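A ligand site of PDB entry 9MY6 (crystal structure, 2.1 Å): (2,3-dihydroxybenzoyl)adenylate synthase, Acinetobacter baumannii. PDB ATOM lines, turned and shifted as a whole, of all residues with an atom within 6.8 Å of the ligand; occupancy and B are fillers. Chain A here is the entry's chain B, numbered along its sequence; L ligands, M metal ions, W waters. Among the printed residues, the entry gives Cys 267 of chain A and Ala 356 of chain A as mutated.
The side-chain sulfur (SG) of Cys 267 lies close to a fluorine (F1) of the ligand.
His 261 touches the ligand.
Phe 263 touches the ligand.
Gly 334 touches the ligand.
Ala 356 touches the ligand (CB to F1, 3.5 Å).
O of Gly 358 touches C2 of the ligand, at 3.4 Å.
Ala 360 touches the ligand.
Val 364 touches the ligand (CG1 to F1, 3.5 Å).
Hydrophobic or aromatic side chains that line the ligand: His 261, Phe 263, Ala 356 and Val 364.
Along chain A the residues within 4 Å of the ligand span positions 261 to 364.
The nearest printed residue that does not touch the ligand is Tyr 366 (4.3 Å).
Water W1 lies within hydrogen-bond range of O2 of the ligand and N of Ala 360.
Water W2 lies within hydrogen-bond range of O1 of the ligand (2.9 Å), O of Gly 358 (3.1 Å) and N of Gly 334 (3.4 Å).
The backbone carbonyl oxygen of Cys 267 sits close to the side-chain hydroxyl of Tyr 366, at 3.5 Å.
The backbone NH (N) of Ala 356 sits at hydrogen-bond distance from the backbone carbonyl oxygen (O) of Val 332.
The side-chain amide nitrogen (ND2) of Asn 262 sits at hydrogen-bond distance from the backbone carbonyl oxygen (O) of Met 359, at 3.4 Å.
N of Phe 263 sits at hydrogen-bond distance from ND1 of His 261 (2.9 Å).
SG of Cys 267 sits close to OG of Ser 266 (3.5 Å).
O of Cys 267 sits at hydrogen-bond distance from NE2 of Gln 331 (2.6 Å).
The backbone carbonyl oxygen (O) of Asn 262 is in hydrogen-bond range of the side-chain hydroxyl (OG) of Ser 266, 3.0 Å away.
O of Asn 262 sits at hydrogen-bond distance from SG of Cys 267.
An oxygen (O3) of the ligand sits at hydrogen-bond distance from the side-chain amide nitrogen of Asn 262, 3.1 Å away.
The backbone NH of Met 359 sits at hydrogen-bond distance from an oxygen (O3) of the ligand, 3.4 Å away.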
ATOM      1  N   LEU A 216     -12.343   4.380  19.320  1.00  0.00           N
ATOM      2  CA  LEU A 216     -11.929   3.882  20.636  1.00  0.00           C
ATOM      3  C   LEU A 216     -13.135   3.894  21.556  1.00  0.00           C
ATOM      4  O   LEU A 216     -13.927   4.835  21.507  1.00  0.00           O
ATOM      5  CB  LEU A 216     -10.814   4.738  21.225  1.00  0.00           C
ATOM      6  CG  LEU A 216      -9.471   4.646  20.519  1.00  0.00           C
ATOM      7  CD1 LEU A 216      -8.382   5.436  21.229  1.00  0.00           C
ATOM      8  CD2 LEU A 216      -9.053   3.176  20.405  1.00  0.00           C
ATOM      9  N   GLY A 218     -15.189   4.282  25.100  1.00  0.00           N
ATOM     10  CA  GLY A 218     -15.109   5.119  26.299  1.00  0.00           C
ATOM     11  C   GLY A 218     -15.572   4.291  27.484  1.00  0.00           C
ATOM     12  O   GLY A 218     -16.550   3.554  27.390  1.00  0.00           O
ATOM     13  N   HIS A 261     -12.314  12.316  18.927  1.00  0.00           N
ATOM     14  CA  HIS A 261     -13.414  11.704  19.669  1.00  0.00           C
ATOM     15  C   HIS A 261     -14.665  11.579  18.791  1.00  0.00           C
ATOM     16  O   HIS A 261     -15.013  12.497  18.042  1.00  0.00           O
ATOM     17  CB  HIS A 261     -13.763  12.549  20.908  1.00  0.00           C
ATOM     18  CG  HIS A 261     -14.691  11.826  21.825  1.00  0.00           C
ATOM     19  ND1 HIS A 261     -16.054  11.750  21.597  1.00  0.00           N
ATOM     20  CD2 HIS A 261     -14.449  11.097  22.944  1.00  0.00           C
ATOM     21  CE1 HIS A 261     -16.609  11.004  22.546  1.00  0.00           C
ATOM     22  NE2 HIS A 261     -15.655  10.582  23.364  1.00  0.00           N
ATOM     23  N   ASN A 262     -15.394  10.462  18.931  1.00  0.00           N
ATOM     24  CA  ASN A 262     -16.561  10.228  18.089  1.00  0.00           C
ATOM     25  C   ASN A 262     -17.509  11.427  18.106  1.00  0.00           C
ATOM     26  O   ASN A 262     -18.041  11.842  17.069  1.00  0.00           O
ATOM     27  CB  ASN A 262     -17.287   8.968  18.567  1.00  0.00           C
ATOM     28  CG  ASN A 262     -18.289   8.432  17.537  1.00  0.00           C
ATOM     29  OD1 ASN A 262     -17.921   8.163  16.384  1.00  0.00           O
ATOM     30  ND2 ASN A 262     -19.549   8.273  17.936  1.00  0.00           N
ATOM     31  N   PHE A 263     -17.739  11.988  19.301  1.00  0.00           N
ATOM     32  CA  PHE A 263     -18.629  13.139  19.456  1.00  0.00           C
ATOM     33  C   PHE A 263     -18.193  14.282  18.540  1.00  0.00           C
ATOM     34  O   PHE A 263     -18.996  14.815  17.765  1.00  0.00           O
ATOM     35  CB  PHE A 263     -18.624  13.588  20.932  1.00  0.00           C
ATOM     36  CG  PHE A 263     -19.682  14.632  21.275  1.00  0.00           C
ATOM     37  CD1 PHE A 263     -20.730  14.920  20.407  1.00  0.00           C
ATOM     38  CD2 PHE A 263     -19.640  15.296  22.502  1.00  0.00           C
ATOM     39  CE1 PHE A 263     -21.716  15.881  20.772  1.00  0.00           C
ATOM     40  CE2 PHE A 263     -20.619  16.242  22.853  1.00  0.00           C
ATOM     41  CZ  PHE A 263     -21.654  16.521  22.001  1.00  0.00           C
ATOM     42  N   MET A 264     -16.905  14.675  18.630  1.00  0.00           N
ATOM     43  CA  MET A 264     -16.369  15.815  17.888  1.00  0.00           C
ATOM     44  C   MET A 264     -16.204  15.514  16.405  1.00  0.00           C
ATOM     45  O   MET A 264     -16.064  16.448  15.609  1.00  0.00           O
ATOM     46  CB  MET A 264     -14.986  16.227  18.420  1.00  0.00           C
ATOM     47  CG  MET A 264     -14.629  17.700  18.252  1.00  0.00           C
ATOM     48  SD  MET A 264     -15.832  18.913  18.918  1.00  0.00           S
ATOM     49  CE  MET A 264     -16.807  19.342  17.460  1.00  0.00           C
ATOM     50  N   SER A 266     -18.086  13.057  14.340  1.00  0.00           N
ATOM     51  CA  SER A 266     -19.203  12.581  13.542  1.00  0.00           C
ATOM     52  C   SER A 266     -20.597  12.874  14.101  1.00  0.00           C
ATOM     53  O   SER A 266     -21.573  12.468  13.455  1.00  0.00           O
ATOM     54  CB  SER A 266     -19.058  11.065  13.335  1.00  0.00           C
ATOM     55  OG  SER A 266     -19.072  10.402  14.596  1.00  0.00           O
ATOM     56  N   CYS A 267     -20.751  13.574  15.222  1.00  0.00           N
ATOM     57  CA  CYS A 267     -22.051  13.634  15.901  1.00  0.00           C
ATOM     58  C   CYS A 267     -22.530  15.056  16.147  1.00  0.00           C
ATOM     59  O   CYS A 267     -22.837  15.423  17.288  1.00  0.00           O
ATOM     60  CB  CYS A 267     -21.981  12.872  17.216  1.00  0.00           C
ATOM     61  SG  CYS A 267     -21.602  11.132  16.976  1.00  0.00           S
ATOM     62  N   PRO A 268     -22.640  15.889  15.118  1.00  0.00           N
ATOM     63  CA  PRO A 268     -22.299  15.659  13.699  1.00  0.00           C
ATOM     64  C   PRO A 268     -20.822  15.900  13.473  1.00  0.00           C
ATOM     65  O   PRO A 268     -20.259  15.401  12.511  1.00  0.00           O
ATOM     66  CB  PRO A 268     -23.154  16.678  12.973  1.00  0.00           C
ATOM     67  CG  PRO A 268     -23.272  17.830  13.974  1.00  0.00           C
ATOM     68  CD  PRO A 268     -23.356  17.165  15.300  1.00  0.00           C
ATOM     69  N   VAL A 306     -18.935  18.627  26.438  1.00  0.00           N
ATOM     70  CA  VAL A 306     -19.323  17.704  27.506  1.00  0.00           C
ATOM     71  C   VAL A 306     -19.787  18.551  28.681  1.00  0.00           C
ATOM     72  O   VAL A 306     -19.455  19.744  28.760  1.00  0.00           O
ATOM     73  CB  VAL A 306     -18.162  16.767  27.918  1.00  0.00           C
ATOM     74  CG1 VAL A 306     -17.770  15.810  26.781  1.00  0.00           C
ATOM     75  CG2 VAL A 306     -16.986  17.555  28.410  1.00  0.00           C
ATOM     76  N   GLN A 331     -24.450  21.470  21.224  1.00  0.00           N
ATOM     77  CA  GLN A 331     -24.734  20.089  21.596  1.00  0.00           C
ATOM     78  C   GLN A 331     -24.017  19.784  22.889  1.00  0.00           C
ATOM     79  O   GLN A 331     -22.870  20.200  23.083  1.00  0.00           O
ATOM     80  CB  GLN A 331     -24.271  19.099  20.546  1.00  0.00           C
ATOM     81  CG  GLN A 331     -24.655  19.405  19.181  1.00  0.00           C
ATOM     82  CD  GLN A 331     -23.865  18.552  18.372  1.00  0.00           C
ATOM     83  OE1 GLN A 331     -22.694  18.865  18.115  1.00  0.00           O
ATOM     84  NE2 GLN A 331     -24.430  17.370  18.018  1.00  0.00           N
ATOM     85  N   VAL A 332     -24.687  19.036  23.766  1.00  0.00           N
ATOM     86  CA  VAL A 332     -24.088  18.616  25.032  1.00  0.00           C
ATOM     87  C   VAL A 332     -24.302  17.123  25.184  1.00  0.00           C
ATOM     88  O   VAL A 332     -25.425  16.636  25.093  1.00  0.00           O
ATOM     89  CB  VAL A 332     -24.675  19.341  26.260  1.00  0.00           C
ATOM     90  CG1 VAL A 332     -23.952  18.787  27.498  1.00  0.00           C
ATOM     91  CG2 VAL A 332     -24.519  20.859  26.149  1.00  0.00           C
ATOM     92  N   GLY A 333     -23.214  16.408  25.473  1.00  0.00           N
ATOM     93  CA  GLY A 333     -23.353  14.978  25.687  1.00  0.00           C
ATOM     94  C   GLY A 333     -22.058  14.503  26.293  1.00  0.00           C
ATOM     95  O   GLY A 333     -21.137  15.293  26.503  1.00  0.00           O
ATOM     96  N   GLY A 334     -22.023  13.206  26.631  1.00  0.00           N
ATOM     97  CA  GLY A 334     -20.809  12.570  27.089  1.00  0.00           C
ATOM     98  C   GLY A 334     -20.724  12.290  28.569  1.00  0.00           C
ATOM     99  O   GLY A 334     -19.795  11.582  28.991  1.00  0.00           O
ATOM    100  N   ALA A 335     -21.650  12.814  29.376  1.00  0.00           N
ATOM    101  CA  ALA A 335     -21.708  12.619  30.829  1.00  0.00           C
ATOM    102  C   ALA A 335     -23.074  13.121  31.255  1.00  0.00           C
ATOM    103  O   ALA A 335     -23.765  13.802  30.492  1.00  0.00           O
ATOM    104  CB  ALA A 335     -20.592  13.356  31.611  1.00  0.00           C
ATOM    105  N   ALA A 356     -27.170  15.124  23.274  1.00  0.00           N
ATOM    106  CA  ALA A 356     -26.696  14.023  22.469  1.00  0.00           C
ATOM    107  C   ALA A 356     -26.230  12.943  23.427  1.00  0.00           C
ATOM    108  O   ALA A 356     -25.548  13.229  24.406  1.00  0.00           O
ATOM    109  CB  ALA A 356     -25.567  14.450  21.530  1.00  0.00           C
ATOM    110  N   PHE A 357     -26.656  11.729  23.174  1.00  0.00           N
ATOM    111  CA  PHE A 357     -26.198  10.564  23.905  1.00  0.00           C
ATOM    112  C   PHE A 357     -25.770   9.572  22.832  1.00  0.00           C
ATOM    113  O   PHE A 357     -26.625   9.050  22.115  1.00  0.00           O
ATOM    114  CB  PHE A 357     -27.325  10.012  24.750  1.00  0.00           C
ATOM    115  CG  PHE A 357     -27.056   8.652  25.243  1.00  0.00           C
ATOM    116  CD1 PHE A 357     -25.814   8.351  25.794  1.00  0.00           C
ATOM    117  CD2 PHE A 357     -28.016   7.649  25.124  1.00  0.00           C
ATOM    118  CE1 PHE A 357     -25.516   7.090  26.251  1.00  0.00           C
ATOM    119  CE2 PHE A 357     -27.747   6.351  25.565  1.00  0.00           C
ATOM    120  CZ  PHE A 357     -26.491   6.075  26.138  1.00  0.00           C
ATOM    121  N   GLY A 358     -24.472   9.316  22.706  1.00  0.00           N
ATOM    122  CA  GLY A 358     -23.955   8.383  21.720  1.00  0.00           C
ATOM    123  C   GLY A 358     -22.817   7.561  22.299  1.00  0.00           C
ATOM    124  O   GLY A 358     -22.462   7.695  23.479  1.00  0.00           O
ATOM    125  N   MET A 359     -22.259   6.690  21.463  1.00  0.00           N
ATOM    126  CA  MET A 359     -21.112   5.897  21.860  1.00  0.00           C
ATOM    127  C   MET A 359     -20.294   5.649  20.599  1.00  0.00           C
ATOM    128  O   MET A 359     -20.855   5.499  19.515  1.00  0.00           O
ATOM    129  CB  MET A 359     -21.542   4.536  22.393  1.00  0.00           C
ATOM    130  CG  MET A 359     -22.803   4.061  21.720  1.00  0.00           C
ATOM    131  SD  MET A 359     -23.454   2.546  22.450  1.00  0.00           S
ATOM    132  CE  MET A 359     -24.784   3.315  23.382  1.00  0.00           C
ATOM    133  N   ALA A 360     -18.976   5.556  20.763  1.00  0.00           N
ATOM    134  CA  ALA A 360     -18.146   5.285  19.603  1.00  0.00           C
ATOM    135  C   ALA A 360     -18.498   3.944  18.959  1.00  0.00           C
ATOM    136  O   ALA A 360     -18.229   3.772  17.776  1.00  0.00           O
ATOM    137  CB  ALA A 360     -16.668   5.354  19.997  1.00  0.00           C
ATOM    138  N   GLU A 361     -19.123   3.018  19.703  1.00  0.00           N
ATOM    139  CA  GLU A 361     -19.531   1.730  19.175  1.00  0.00           C
ATOM    140  C   GLU A 361     -20.631   1.843  18.133  1.00  0.00           C
ATOM    141  O   GLU A 361     -20.834   0.894  17.361  1.00  0.00           O
ATOM    142  CB  GLU A 361     -19.973   0.779  20.287  1.00  0.00           C
ATOM    143  CG  GLU A 361     -18.803   0.262  21.096  1.00  0.00           C
ATOM    144  CD  GLU A 361     -18.390   1.186  22.271  1.00  0.00           C
ATOM    145  OE1 GLU A 361     -18.808   2.376  22.311  1.00  0.00           O
ATOM    146  OE2 GLU A 361     -17.536   0.772  23.091  1.00  0.00           O
ATOM    147  N   GLY A 362     -21.302   2.998  18.042  1.00  0.00           N
ATOM    148  CA  GLY A 362     -22.385   3.156  17.079  1.00  0.00           C
ATOM    149  C   GLY A 362     -23.476   4.120  17.527  1.00  0.00           C
ATOM    150  O   GLY A 362     -23.344   5.326  17.355  1.00  0.00           O
ATOM    151  N   LEU A 363     -24.542   3.592  18.140  1.00  0.00           N
ATOM    152  CA  LEU A 363     -25.789   4.323  18.359  1.00  0.00           C
ATOM    153  C   LEU A 363     -25.550   5.744  18.857  1.00  0.00           C
ATOM    154  O   LEU A 363     -24.804   5.973  19.812  1.00  0.00           O
ATOM    155  CB  LEU A 363     -26.621   3.565  19.399  1.00  0.00           C
ATOM    156  CG  LEU A 363     -27.921   4.221  19.875  1.00  0.00           C
ATOM    157  CD1 LEU A 363     -28.953   4.194  18.705  1.00  0.00           C
ATOM    158  CD2 LEU A 363     -28.432   3.530  21.123  1.00  0.00           C
ATOM    159  N   VAL A 364     -26.245   6.701  18.226  1.00  0.00           N
ATOM    160  CA  VAL A 364     -26.262   8.100  18.620  1.00  0.00           C
ATOM    161  C   VAL A 364     -27.697   8.570  18.723  1.00  0.00           C
ATOM    162  O   VAL A 364     -28.489   8.335  17.813  1.00  0.00           O
ATOM    163  CB  VAL A 364     -25.486   8.989  17.646  1.00  0.00           C
ATOM    164  CG1 VAL A 364     -25.450  10.446  18.215  1.00  0.00           C
ATOM    165  CG2 VAL A 364     -24.102   8.460  17.525  1.00  0.00           C
ATOM    166  N   ASN A 365     -28.036   9.248  19.832  1.00  0.00           N
ATOM    167  CA  ASN A 365     -29.332   9.857  20.052  1.00  0.00           C
ATOM    168  C   ASN A 365     -29.178  11.365  20.146  1.00  0.00           C
ATOM    169  O   ASN A 365     -28.189  11.859  20.683  1.00  0.00           O
ATOM    170  CB  ASN A 365     -29.966   9.330  21.325  1.00  0.00           C
ATOM    171  CG  ASN A 365     -30.043   7.825  21.346  1.00  0.00           C
ATOM    172  OD1 ASN A 365     -31.083   7.246  21.048  1.00  0.00           O
ATOM    173  ND2 ASN A 365     -28.938   7.176  21.725  1.00  0.00           N
ATOM    174  N   TYR A 366     -30.131  12.091  19.580  1.00  0.00           N
ATOM    175  CA  TYR A 366     -30.199  13.538  19.658  1.00  0.00           C
ATOM    176  C   TYR A 366     -31.606  13.943  20.006  1.00  0.00           C
ATOM    177  O   TYR A 366     -32.561  13.324  19.510  1.00  0.00           O
ATOM    178  CB  TYR A 366     -29.880  14.246  18.347  1.00  0.00           C
ATOM    179  CG  TYR A 366     -28.569  13.934  17.736  1.00  0.00           C
ATOM    180  CD1 TYR A 366     -27.407  14.528  18.200  1.00  0.00           C
ATOM    181  CD2 TYR A 366     -28.487  13.065  16.628  1.00  0.00           C
ATOM    182  CE1 TYR A 366     -26.174  14.244  17.616  1.00  0.00           C
ATOM    183  CE2 TYR A 366     -27.291  12.776  16.044  1.00  0.00           C
ATOM    184  CZ  TYR A 366     -26.136  13.364  16.510  1.00  0.00           C
ATOM    185  OH  TYR A 366     -24.965  13.059  15.889  1.00  0.00           O
HETATM  186  C1  LIG L   1     -20.686  10.076  21.382  1.00  0.00           C
HETATM  187  C2  LIG L   1     -19.749   9.673  23.617  1.00  0.00           C
HETATM  188  C3  LIG L   1     -20.664  10.456  22.703  1.00  0.00           C
HETATM  189  C4  LIG L   1     -21.478  11.477  23.171  1.00  0.00           C
HETATM  190  C5  LIG L   1     -22.308  12.126  22.271  1.00  0.00           C
HETATM  191  C6  LIG L   1     -22.330  11.746  20.951  1.00  0.00           C
HETATM  192  C7  LIG L   1     -21.518  10.721  20.507  1.00  0.00           C
HETATM  193  F1  LIG L   1     -23.154  12.392  20.064  1.00  0.00           F
HETATM  194  O1  LIG L   1     -19.850   9.834  24.838  1.00  0.00           O
HETATM  195  O2  LIG L   1     -18.931   8.833  23.116  1.00  0.00           O
HETATM  196  O3  LIG L   1     -19.850   9.020  20.976  1.00  0.00           O
HETATM  197 CA    CA M   1     -19.243   3.417  26.516  1.00  0.00          CA
HETATM  198  O   HOH W   1     -17.789   6.538  23.246  1.00  0.00           O
HETATM  199  O   HOH W   2     -22.640  10.073  25.436  1.00  0.00           O
